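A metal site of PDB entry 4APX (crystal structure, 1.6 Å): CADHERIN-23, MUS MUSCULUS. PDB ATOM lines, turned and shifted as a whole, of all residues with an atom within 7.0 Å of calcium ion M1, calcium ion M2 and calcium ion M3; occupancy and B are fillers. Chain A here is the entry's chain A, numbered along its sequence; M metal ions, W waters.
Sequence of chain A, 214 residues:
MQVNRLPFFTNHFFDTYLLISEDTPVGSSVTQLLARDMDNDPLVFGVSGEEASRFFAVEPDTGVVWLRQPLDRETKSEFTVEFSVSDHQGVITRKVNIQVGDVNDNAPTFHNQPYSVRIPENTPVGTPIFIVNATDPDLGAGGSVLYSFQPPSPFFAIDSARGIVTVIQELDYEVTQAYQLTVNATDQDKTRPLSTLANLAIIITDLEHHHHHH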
ATOM      1  N   GLU A  22       8.683  31.579 -28.378  1.00  0.00           N
ATOM      2  CA  GLU A  22       9.063  31.474 -29.802  1.00  0.00           C
ATOM      3  C   GLU A  22       8.192  30.525 -30.639  1.00  0.00           C
ATOM      4  O   GLU A  22       8.241  30.616 -31.861  1.00  0.00           O
ATOM      5  CB  GLU A  22      10.554  31.098 -29.976  1.00  0.00           C
ATOM      6  CG  GLU A  22      10.905  29.729 -29.500  1.00  0.00           C
ATOM      7  CD  GLU A  22      12.325  29.336 -29.825  1.00  0.00           C
ATOM      8  OE1 GLU A  22      12.865  29.832 -30.869  1.00  0.00           O
ATOM      9  OE2 GLU A  22      12.885  28.502 -29.069  1.00  0.00           O
ATOM     10  N   LEU A  71       8.786  34.046 -34.553  1.00  0.00           N
ATOM     11  CA  LEU A  71       9.866  34.460 -33.678  1.00  0.00           C
ATOM     12  C   LEU A  71      10.870  33.308 -33.645  1.00  0.00           C
ATOM     13  O   LEU A  71      10.551  32.175 -34.035  1.00  0.00           O
ATOM     14  CB  LEU A  71       9.355  34.773 -32.271  1.00  0.00           C
ATOM     15  CG  LEU A  71       8.428  35.976 -32.096  1.00  0.00           C
ATOM     16  CD1 LEU A  71       7.836  35.987 -30.695  1.00  0.00           C
ATOM     17  CD2 LEU A  71       9.125  37.288 -32.380  1.00  0.00           C
ATOM     18  N   ASP A  72      12.103  33.597 -33.278  1.00  0.00           N
ATOM     19  CA  ASP A  72      13.131  32.553 -33.153  1.00  0.00           C
ATOM     20  C   ASP A  72      14.126  33.038 -32.141  1.00  0.00           C
ATOM     21  O   ASP A  72      14.962  33.879 -32.453  1.00  0.00           O
ATOM     22  CB  ASP A  72      13.809  32.254 -34.505  1.00  0.00           C
ATOM     23  CG  ASP A  72      14.956  31.271 -34.371  1.00  0.00           C
ATOM     24  OD1 ASP A  72      15.075  30.610 -33.305  1.00  0.00           O
ATOM     25  OD2 ASP A  72      15.740  31.149 -35.319  1.00  0.00           O
ATOM     26  N   ARG A  73      14.060  32.474 -30.929  1.00  0.00           N
ATOM     27  CA  ARG A  73      14.898  32.886 -29.839  1.00  0.00           C
ATOM     28  C   ARG A  73      16.386  32.719 -30.161  1.00  0.00           C
ATOM     29  O   ARG A  73      17.220  33.481 -29.673  1.00  0.00           O
ATOM     30  CB  ARG A  73      14.578  32.100 -28.573  1.00  0.00           C
ATOM     31  CG  ARG A  73      15.205  32.703 -27.314  1.00  0.00           C
ATOM     32  CD  ARG A  73      15.346  31.757 -26.193  1.00  0.00           C
ATOM     33  NE  ARG A  73      16.325  30.720 -26.549  1.00  0.00           N
ATOM     34  CZ  ARG A  73      17.640  30.823 -26.400  1.00  0.00           C
ATOM     35  NH1 ARG A  73      18.216  31.881 -25.831  1.00  0.00           N
ATOM     36  NH2 ARG A  73      18.400  29.820 -26.808  1.00  0.00           N
ATOM     37  N   GLU A  74      16.698  31.711 -30.980  1.00  0.00           N
ATOM     38  CA  GLU A  74      18.083  31.456 -31.386  1.00  0.00           C
ATOM     39  C   GLU A  74      18.587  32.448 -32.450  1.00  0.00           C
ATOM     40  O   GLU A  74      19.818  32.524 -32.679  1.00  0.00           O
ATOM     41  CB  GLU A  74      18.233  30.026 -31.892  1.00  0.00           C
ATOM     42  CG  GLU A  74      18.272  28.965 -30.808  1.00  0.00           C
ATOM     43  CD  GLU A  74      16.919  28.681 -30.166  1.00  0.00           C
ATOM     44  OE1 GLU A  74      15.887  28.577 -30.862  1.00  0.00           O
ATOM     45  OE2 GLU A  74      16.896  28.438 -28.937  1.00  0.00           O
ATOM     46  N   THR A  75      17.681  33.167 -33.119  1.00  0.00           N
ATOM     47  CA  THR A  75      18.058  34.192 -34.137  1.00  0.00           C
ATOM     48  C   THR A  75      18.004  35.586 -33.498  1.00  0.00           C
ATOM     49  O   THR A  75      18.884  36.429 -33.745  1.00  0.00           O
ATOM     50  CB  THR A  75      17.166  34.125 -35.396  1.00  0.00           C
ATOM     51  OG1 THR A  75      17.501  32.946 -36.141  1.00  0.00           O
ATOM     52  CG2 THR A  75      17.394  35.324 -36.305  1.00  0.00           C
ATOM     53  N   GLY A 101      10.531  33.727 -25.391  1.00  0.00           N
ATOM     54  CA  GLY A 101      10.652  32.538 -24.567  1.00  0.00           C
ATOM     55  C   GLY A 101      11.170  31.364 -25.377  1.00  0.00           C
ATOM     56  O   GLY A 101      10.855  31.230 -26.563  1.00  0.00           O
ATOM     57  N   ASP A 102      11.966  30.518 -24.748  1.00  0.00           N
ATOM     58  CA  ASP A 102      12.554  29.389 -25.455  1.00  0.00           C
ATOM     59  C   ASP A 102      11.652  28.173 -25.476  1.00  0.00           C
ATOM     60  O   ASP A 102      10.896  27.927 -24.527  1.00  0.00           O
ATOM     61  CB  ASP A 102      13.884  28.970 -24.794  1.00  0.00           C
ATOM     62  CG  ASP A 102      14.662  27.972 -25.626  1.00  0.00           C
ATOM     63  OD1 ASP A 102      14.914  28.240 -26.833  1.00  0.00           O
ATOM     64  OD2 ASP A 102      15.037  26.907 -25.107  1.00  0.00           O
ATOM     65  N   VAL A 103      11.723  27.437 -26.572  1.00  0.00           N
ATOM     66  CA  VAL A 103      11.220  26.077 -26.607  1.00  0.00           C
ATOM     67  C   VAL A 103      12.336  25.223 -27.176  1.00  0.00           C
ATOM     68  O   VAL A 103      13.240  25.735 -27.823  1.00  0.00           O
ATOM     69  CB  VAL A 103       9.933  25.907 -27.375  1.00  0.00           C
ATOM     70  CG1 VAL A 103       8.842  26.861 -26.869  1.00  0.00           C
ATOM     71  CG2 VAL A 103      10.163  26.106 -28.859  1.00  0.00           C
ATOM     72  N   ASN A 104      12.309  23.931 -26.899  1.00  0.00           N
ATOM     73  CA  ASN A 104      13.320  23.039 -27.472  1.00  0.00           C
ATOM     74  C   ASN A 104      12.985  22.826 -28.937  1.00  0.00           C
ATOM     75  O   ASN A 104      12.054  22.087 -29.265  1.00  0.00           O
ATOM     76  CB  ASN A 104      13.392  21.702 -26.717  1.00  0.00           C
ATOM     77  CG  ASN A 104      14.560  20.875 -27.175  1.00  0.00           C
ATOM     78  OD1 ASN A 104      15.670  21.404 -27.224  1.00  0.00           O
ATOM     79  ND2 ASN A 104      14.332  19.632 -27.576  1.00  0.00           N
ATOM     80  N   ASP A 105      13.717  23.515 -29.812  1.00  0.00           N
ATOM     81  CA  ASP A 105      13.453  23.379 -31.249  1.00  0.00           C
ATOM     82  C   ASP A 105      14.682  23.129 -32.103  1.00  0.00           C
ATOM     83  O   ASP A 105      14.584  23.154 -33.347  1.00  0.00           O
ATOM     84  CB  ASP A 105      12.564  24.522 -31.793  1.00  0.00           C
ATOM     85  CG  ASP A 105      13.146  25.912 -31.615  1.00  0.00           C
ATOM     86  OD1 ASP A 105      14.161  26.085 -30.918  1.00  0.00           O
ATOM     87  OD2 ASP A 105      12.572  26.883 -32.196  1.00  0.00           O
ATOM     88  N   ASN A 106      15.820  22.831 -31.466  1.00  0.00           N
ATOM     89  CA  ASN A 106      17.024  22.435 -32.154  1.00  0.00           C
ATOM     90  C   ASN A 106      17.526  21.085 -31.674  1.00  0.00           C
ATOM     91  O   ASN A 106      17.462  20.776 -30.490  1.00  0.00           O
ATOM     92  CB  ASN A 106      18.172  23.448 -31.955  1.00  0.00           C
ATOM     93  CG  ASN A 106      17.865  24.786 -32.565  1.00  0.00           C
ATOM     94  OD1 ASN A 106      18.295  25.059 -33.707  1.00  0.00           O
ATOM     95  ND2 ASN A 106      17.089  25.626 -31.861  1.00  0.00           N
ATOM     96  N   ALA A 107      18.045  20.306 -32.611  1.00  0.00           N
ATOM     97  CA  ALA A 107      18.741  19.082 -32.287  1.00  0.00           C
ATOM     98  C   ALA A 107      20.216  19.429 -32.157  1.00  0.00           C
ATOM     99  O   ALA A 107      20.664  20.469 -32.668  1.00  0.00           O
ATOM    100  CB  ALA A 107      18.539  18.008 -33.350  1.00  0.00           C
ATOM    101  N   PRO A 108      20.998  18.570 -31.470  1.00  0.00           N
ATOM    102  CA  PRO A 108      22.438  18.833 -31.397  1.00  0.00           C
ATOM    103  C   PRO A 108      23.160  18.775 -32.745  1.00  0.00           C
ATOM    104  O   PRO A 108      22.693  18.136 -33.693  1.00  0.00           O
ATOM    105  CB  PRO A 108      22.964  17.725 -30.477  1.00  0.00           C
ATOM    106  CG  PRO A 108      21.742  17.297 -29.687  1.00  0.00           C
ATOM    107  CD  PRO A 108      20.610  17.423 -30.626  1.00  0.00           C
ATOM    108  N   ASP A 136      24.227  22.262 -28.634  1.00  0.00           N
ATOM    109  CA  ASP A 136      22.803  22.477 -28.868  1.00  0.00           C
ATOM    110  C   ASP A 136      22.426  23.815 -28.273  1.00  0.00           C
ATOM    111  O   ASP A 136      22.677  24.036 -27.078  1.00  0.00           O
ATOM    112  CB  ASP A 136      22.053  21.325 -28.206  1.00  0.00           C
ATOM    113  CG  ASP A 136      20.542  21.325 -28.484  1.00  0.00           C
ATOM    114  OD1 ASP A 136      19.894  22.410 -28.491  1.00  0.00           O
ATOM    115  OD2 ASP A 136      19.973  20.219 -28.654  1.00  0.00           O
ATOM    116  N   PRO A 137      21.843  24.722 -29.079  1.00  0.00           N
ATOM    117  CA  PRO A 137      21.611  26.103 -28.659  1.00  0.00           C
ATOM    118  C   PRO A 137      20.401  26.398 -27.796  1.00  0.00           C
ATOM    119  O   PRO A 137      20.265  27.522 -27.310  1.00  0.00           O
ATOM    120  CB  PRO A 137      21.464  26.840 -30.000  1.00  0.00           C
ATOM    121  CG  PRO A 137      20.792  25.854 -30.869  1.00  0.00           C
ATOM    122  CD  PRO A 137      21.485  24.539 -30.501  1.00  0.00           C
ATOM    123  N   ASP A 138      19.529  25.419 -27.601  1.00  0.00           N
ATOM    124  CA  ASP A 138      18.344  25.633 -26.780  1.00  0.00           C
ATOM    125  C   ASP A 138      18.736  25.790 -25.330  1.00  0.00           C
ATOM    126  O   ASP A 138      19.841  25.404 -24.935  1.00  0.00           O
ATOM    127  CB  ASP A 138      17.404  24.469 -26.938  1.00  0.00           C
ATOM    128  CG  ASP A 138      16.819  24.359 -28.344  1.00  0.00           C
ATOM    129  OD1 ASP A 138      16.203  25.337 -28.835  1.00  0.00           O
ATOM    130  OD2 ASP A 138      16.964  23.283 -28.922  1.00  0.00           O
ATOM    131  N   LEU A 139      17.840  26.354 -24.530  1.00  0.00           N
ATOM    132  CA  LEU A 139      18.133  26.595 -23.114  1.00  0.00           C
ATOM    133  C   LEU A 139      17.934  25.377 -22.237  1.00  0.00           C
ATOM    134  O   LEU A 139      17.110  24.486 -22.543  1.00  0.00           O
ATOM    135  CB  LEU A 139      17.243  27.721 -22.563  1.00  0.00           C
ATOM    136  CG  LEU A 139      17.401  29.134 -23.145  1.00  0.00           C
ATOM    137  CD1 LEU A 139      16.518  30.153 -22.429  1.00  0.00           C
ATOM    138  CD2 LEU A 139      18.857  29.549 -23.086  1.00  0.00           C
ATOM    139  N   ALA A 141      17.655  22.089 -20.162  1.00  0.00           N
ATOM    140  CA  ALA A 141      17.733  20.668 -20.509  1.00  0.00           C
ATOM    141  C   ALA A 141      17.753  20.459 -22.008  1.00  0.00           C
ATOM    142  O   ALA A 141      18.409  19.546 -22.510  1.00  0.00           O
ATOM    143  CB  ALA A 141      16.571  19.902 -19.873  1.00  0.00           C
ATOM    144  N   GLY A 142      17.049  21.312 -22.730  1.00  0.00           N
ATOM    145  CA  GLY A 142      17.058  21.304 -24.196  1.00  0.00           C
ATOM    146  C   GLY A 142      18.385  21.573 -24.853  1.00  0.00           C
ATOM    147  O   GLY A 142      18.538  21.311 -26.045  1.00  0.00           O
ATOM    148  N   GLY A 143      19.364  22.083 -24.101  1.00  0.00           N
ATOM    149  CA  GLY A 143      20.687  22.339 -24.608  1.00  0.00           C
ATOM    150  C   GLY A 143      21.784  21.475 -24.030  1.00  0.00           C
ATOM    151  O   GLY A 143      22.961  21.683 -24.333  1.00  0.00           O
ATOM    152  N   SER A 144      21.420  20.519 -23.173  1.00  0.00           N
ATOM    153  CA  SER A 144      22.389  19.657 -22.482  1.00  0.00           C
ATOM    154  C   SER A 144      22.404  18.325 -23.186  1.00  0.00           C
ATOM    155  O   SER A 144      21.387  17.639 -23.247  1.00  0.00           O
ATOM    156  CB  SER A 144      22.012  19.515 -21.010  1.00  0.00           C
ATOM    157  OG  SER A 144      22.967  18.740 -20.295  1.00  0.00           O
ATOM    158  N   THR A 186      21.765  13.437 -28.011  1.00  0.00           N
ATOM    159  CA  THR A 186      20.402  13.915 -27.728  1.00  0.00           C
ATOM    160  C   THR A 186      20.420  14.998 -26.699  1.00  0.00           C
ATOM    161  O   THR A 186      21.255  15.011 -25.809  1.00  0.00           O
ATOM    162  CB  THR A 186      19.476  12.762 -27.232  1.00  0.00           C
ATOM    163  OG1 THR A 186      18.129  13.243 -27.090  1.00  0.00           O
ATOM    164  CG2 THR A 186      19.953  12.193 -25.878  1.00  0.00           C
ATOM    165  N   ASP A 187      19.495  15.952 -26.811  1.00  0.00           N
ATOM    166  CA  ASP A 187      19.266  16.867 -25.717  1.00  0.00           C
ATOM    167  C   ASP A 187      18.379  16.146 -24.686  1.00  0.00           C
ATOM    168  O   ASP A 187      18.007  14.973 -24.903  1.00  0.00           O
ATOM    169  CB  ASP A 187      18.699  18.218 -26.171  1.00  0.00           C
ATOM    170  CG  ASP A 187      17.368  18.120 -26.808  1.00  0.00           C
ATOM    171  OD1 ASP A 187      16.527  17.348 -26.332  1.00  0.00           O
ATOM    172  OD2 ASP A 187      17.136  18.866 -27.798  1.00  0.00           O
ATOM    173  N   GLN A 188      18.092  16.823 -23.576  1.00  0.00           N
ATOM    174  CA  GLN A 188      17.340  16.231 -22.472  1.00  0.00           C
ATOM    175  C   GLN A 188      15.999  16.925 -22.203  1.00  0.00           C
ATOM    176  O   GLN A 188      15.482  16.894 -21.088  1.00  0.00           O
ATOM    177  CB  GLN A 188      18.206  16.238 -21.215  1.00  0.00           C
ATOM    178  CG  GLN A 188      19.416  15.344 -21.356  1.00  0.00           C
ATOM    179  CD  GLN A 188      20.304  15.420 -20.167  1.00  0.00           C
ATOM    180  OE1 GLN A 188      20.075  14.729 -19.162  1.00  0.00           O
ATOM    181  NE2 GLN A 188      21.327  16.275 -20.249  1.00  0.00           N
ATOM    182  N   ASP A 189      15.417  17.510 -23.226  1.00  0.00           N
ATOM    183  CA  ASP A 189      14.133  18.155 -23.082  1.00  0.00           C
ATOM    184  C   ASP A 189      13.124  17.126 -22.581  1.00  0.00           C
ATOM    185  O   ASP A 189      13.114  15.990 -23.039  1.00  0.00           O
ATOM    186  CB  ASP A 189      13.627  18.768 -24.369  1.00  0.00           C
ATOM    187  CG  ASP A 189      12.360  19.564 -24.158  1.00  0.00           C
ATOM    188  OD1 ASP A 189      12.407  20.582 -23.411  1.00  0.00           O
ATOM    189  OD2 ASP A 189      11.311  19.161 -24.703  1.00  0.00           O
ATOM    190  N   ARG A 192       9.875  16.926 -25.548  1.00  0.00           N
ATOM    191  CA  ARG A 192      10.240  16.838 -26.969  1.00  0.00           C
ATOM    192  C   ARG A 192      11.759  16.815 -27.152  1.00  0.00           C
ATOM    193  O   ARG A 192      12.324  17.724 -27.768  1.00  0.00           O
ATOM    194  CB  ARG A 192       9.634  17.998 -27.754  1.00  0.00           C
ATOM    195  CG  ARG A 192       8.079  18.011 -27.779  1.00  0.00           C
ATOM    196  CD  ARG A 192       7.480  19.131 -28.631  1.00  0.00           C
ATOM    197  NE  ARG A 192       7.947  19.114 -30.002  1.00  0.00           N
ATOM    198  CZ  ARG A 192       8.974  19.813 -30.497  1.00  0.00           C
ATOM    199  NH1 ARG A 192       9.660  20.662 -29.731  1.00  0.00           N
ATOM    200  NH2 ARG A 192       9.319  19.644 -31.760  1.00  0.00           N
ATOM    201  N   PRO A 193      12.411  15.772 -26.649  1.00  0.00           N
ATOM    202  CA  PRO A 193      13.843  15.658 -26.864  1.00  0.00           C
ATOM    203  C   PRO A 193      14.183  15.489 -28.352  1.00  0.00           C
ATOM    204  O   PRO A 193      13.446  14.830 -29.080  1.00  0.00           O
ATOM    205  CB  PRO A 193      14.213  14.407 -26.092  1.00  0.00           C
ATOM    206  CG  PRO A 193      12.947  13.563 -26.169  1.00  0.00           C
ATOM    207  CD  PRO A 193      11.876  14.577 -25.957  1.00  0.00           C
ATOM    208  N   LEU A 194      15.270  16.118 -28.763  1.00  0.00           N
ATOM    209  CA  LEU A 194      15.709  16.084 -30.139  1.00  0.00           C
ATOM    210  C   LEU A 194      17.118  15.523 -30.198  1.00  0.00           C
ATOM    211  O   LEU A 194      17.927  15.769 -29.311  1.00  0.00           O
ATOM    212  CB  LEU A 194      15.648  17.476 -30.751  1.00  0.00           C
ATOM    213  CG  LEU A 194      14.225  18.048 -30.854  1.00  0.00           C
ATOM    214  CD1 LEU A 194      14.277  19.484 -31.288  1.00  0.00           C
ATOM    215  CD2 LEU A 194      13.367  17.221 -31.792  1.00  0.00           C
HETATM  216 CA    CA M   1      14.173  28.621 -32.419  1.00  0.00          CA
HETATM  217 CA    CA M   2      14.836  27.180 -28.891  1.00  0.00          CA
HETATM  218 CA    CA M   3      17.810  21.118 -28.259  1.00  0.00          CA
HETATM  219  O   HOH W   1      15.593  27.374 -33.876  1.00  0.00           O
HETATM  220  O   HOH W   2      12.726  29.073 -34.273  1.00  0.00           O
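The nearest printed residue that does not touch calcium ion M3 is Ala 107 (4.4 Å).
OD2 of Asp 72 lies within hydrogen-bond range of OG1 of Thr 75, at 2.6 Å.
The side-chain amide nitrogen of Asn 106 lies close to the side-chain carboxylate of Asp 105, 3.1 Å away.
OD2 of Asp 102 sits at hydrogen-bond distance from N of Leu 139 (2.9 Å).
ND2 of Asn 104 sits at hydrogen-bond distance from O of Arg 192, at 2.8 Å.
N of Asp 189 is in hydrogen-bond range of OD1 of Asp 187 (3.3 Å).
The side-chain carboxylate (OE2) of Glu 74 sits close to the guanidinium group (NH2) of Arg 73 (3.0 Å).
The backbone NH (N) of Gly 143 lies close to the backbone carbonyl oxygen (O) of Asp 138.
The backbone carbonyl oxygen (O) of Gly 101 lies within hydrogen-bond range of the backbone NH (N) of Glu 22, at 2.9 Å.
Calcium ion M2 is bound by OD1 of Asp 138 (2.3 Å), OD1 of Asp 102 (2.3 Å), OE2 of Glu 22 (2.4 Å), OD1 of Asp 105 (2.4 Å), O of Val 103 (2.4 Å), OE2 of Glu 74 (2.4 Å) and OE1 of Glu 74 (2.6 Å).
Four residues have an atom within 4 Å of calcium ion M1: Glu 22, Asp 72, Glu 74 and Asp 105.
The nearest printed residue that does not touch calcium ion M1 is Arg 73 (4.1 Å).
Calcium ion M3 is bound by the backbone carbonyl oxygen (O) of Asn 106 (2.3 Å), the backbone carbonyl oxygen (O) of Gly 142 (2.3 Å), the side-chain carboxylate (OD2) of Asp 136 (2.4 Å), the side-chain amide oxygen (OD1) of Asn 104 (2.4 Å), the side-chain carboxylate (OD2) of Asp 187 (2.4 Å), the side-chain carboxylate (OD2) of Asp 138 (2.4 Å) and the side-chain carboxylate (OD1) of Asp 136 (2.5 Å).
Calcium ion M1 is bound by the side-chain carboxylate (OE1) of Glu 74.
OD1 of Asp 72 is bound to calcium ion M1, at 2.4 Å.
Calcium ion M1 is bound by OE1 of Glu 22 (2.4 Å).
OD2 of Asp 105 is bound to calcium ion M1 (2.4 Å).
Water W1 is bound to calcium ion M1 (2.4 Å).
Water W2 is bound to calcium ion M1 (2.4 Å).
Slightly farther from calcium ion M1 lies OD1 of Asp 105 (2.9 Å).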
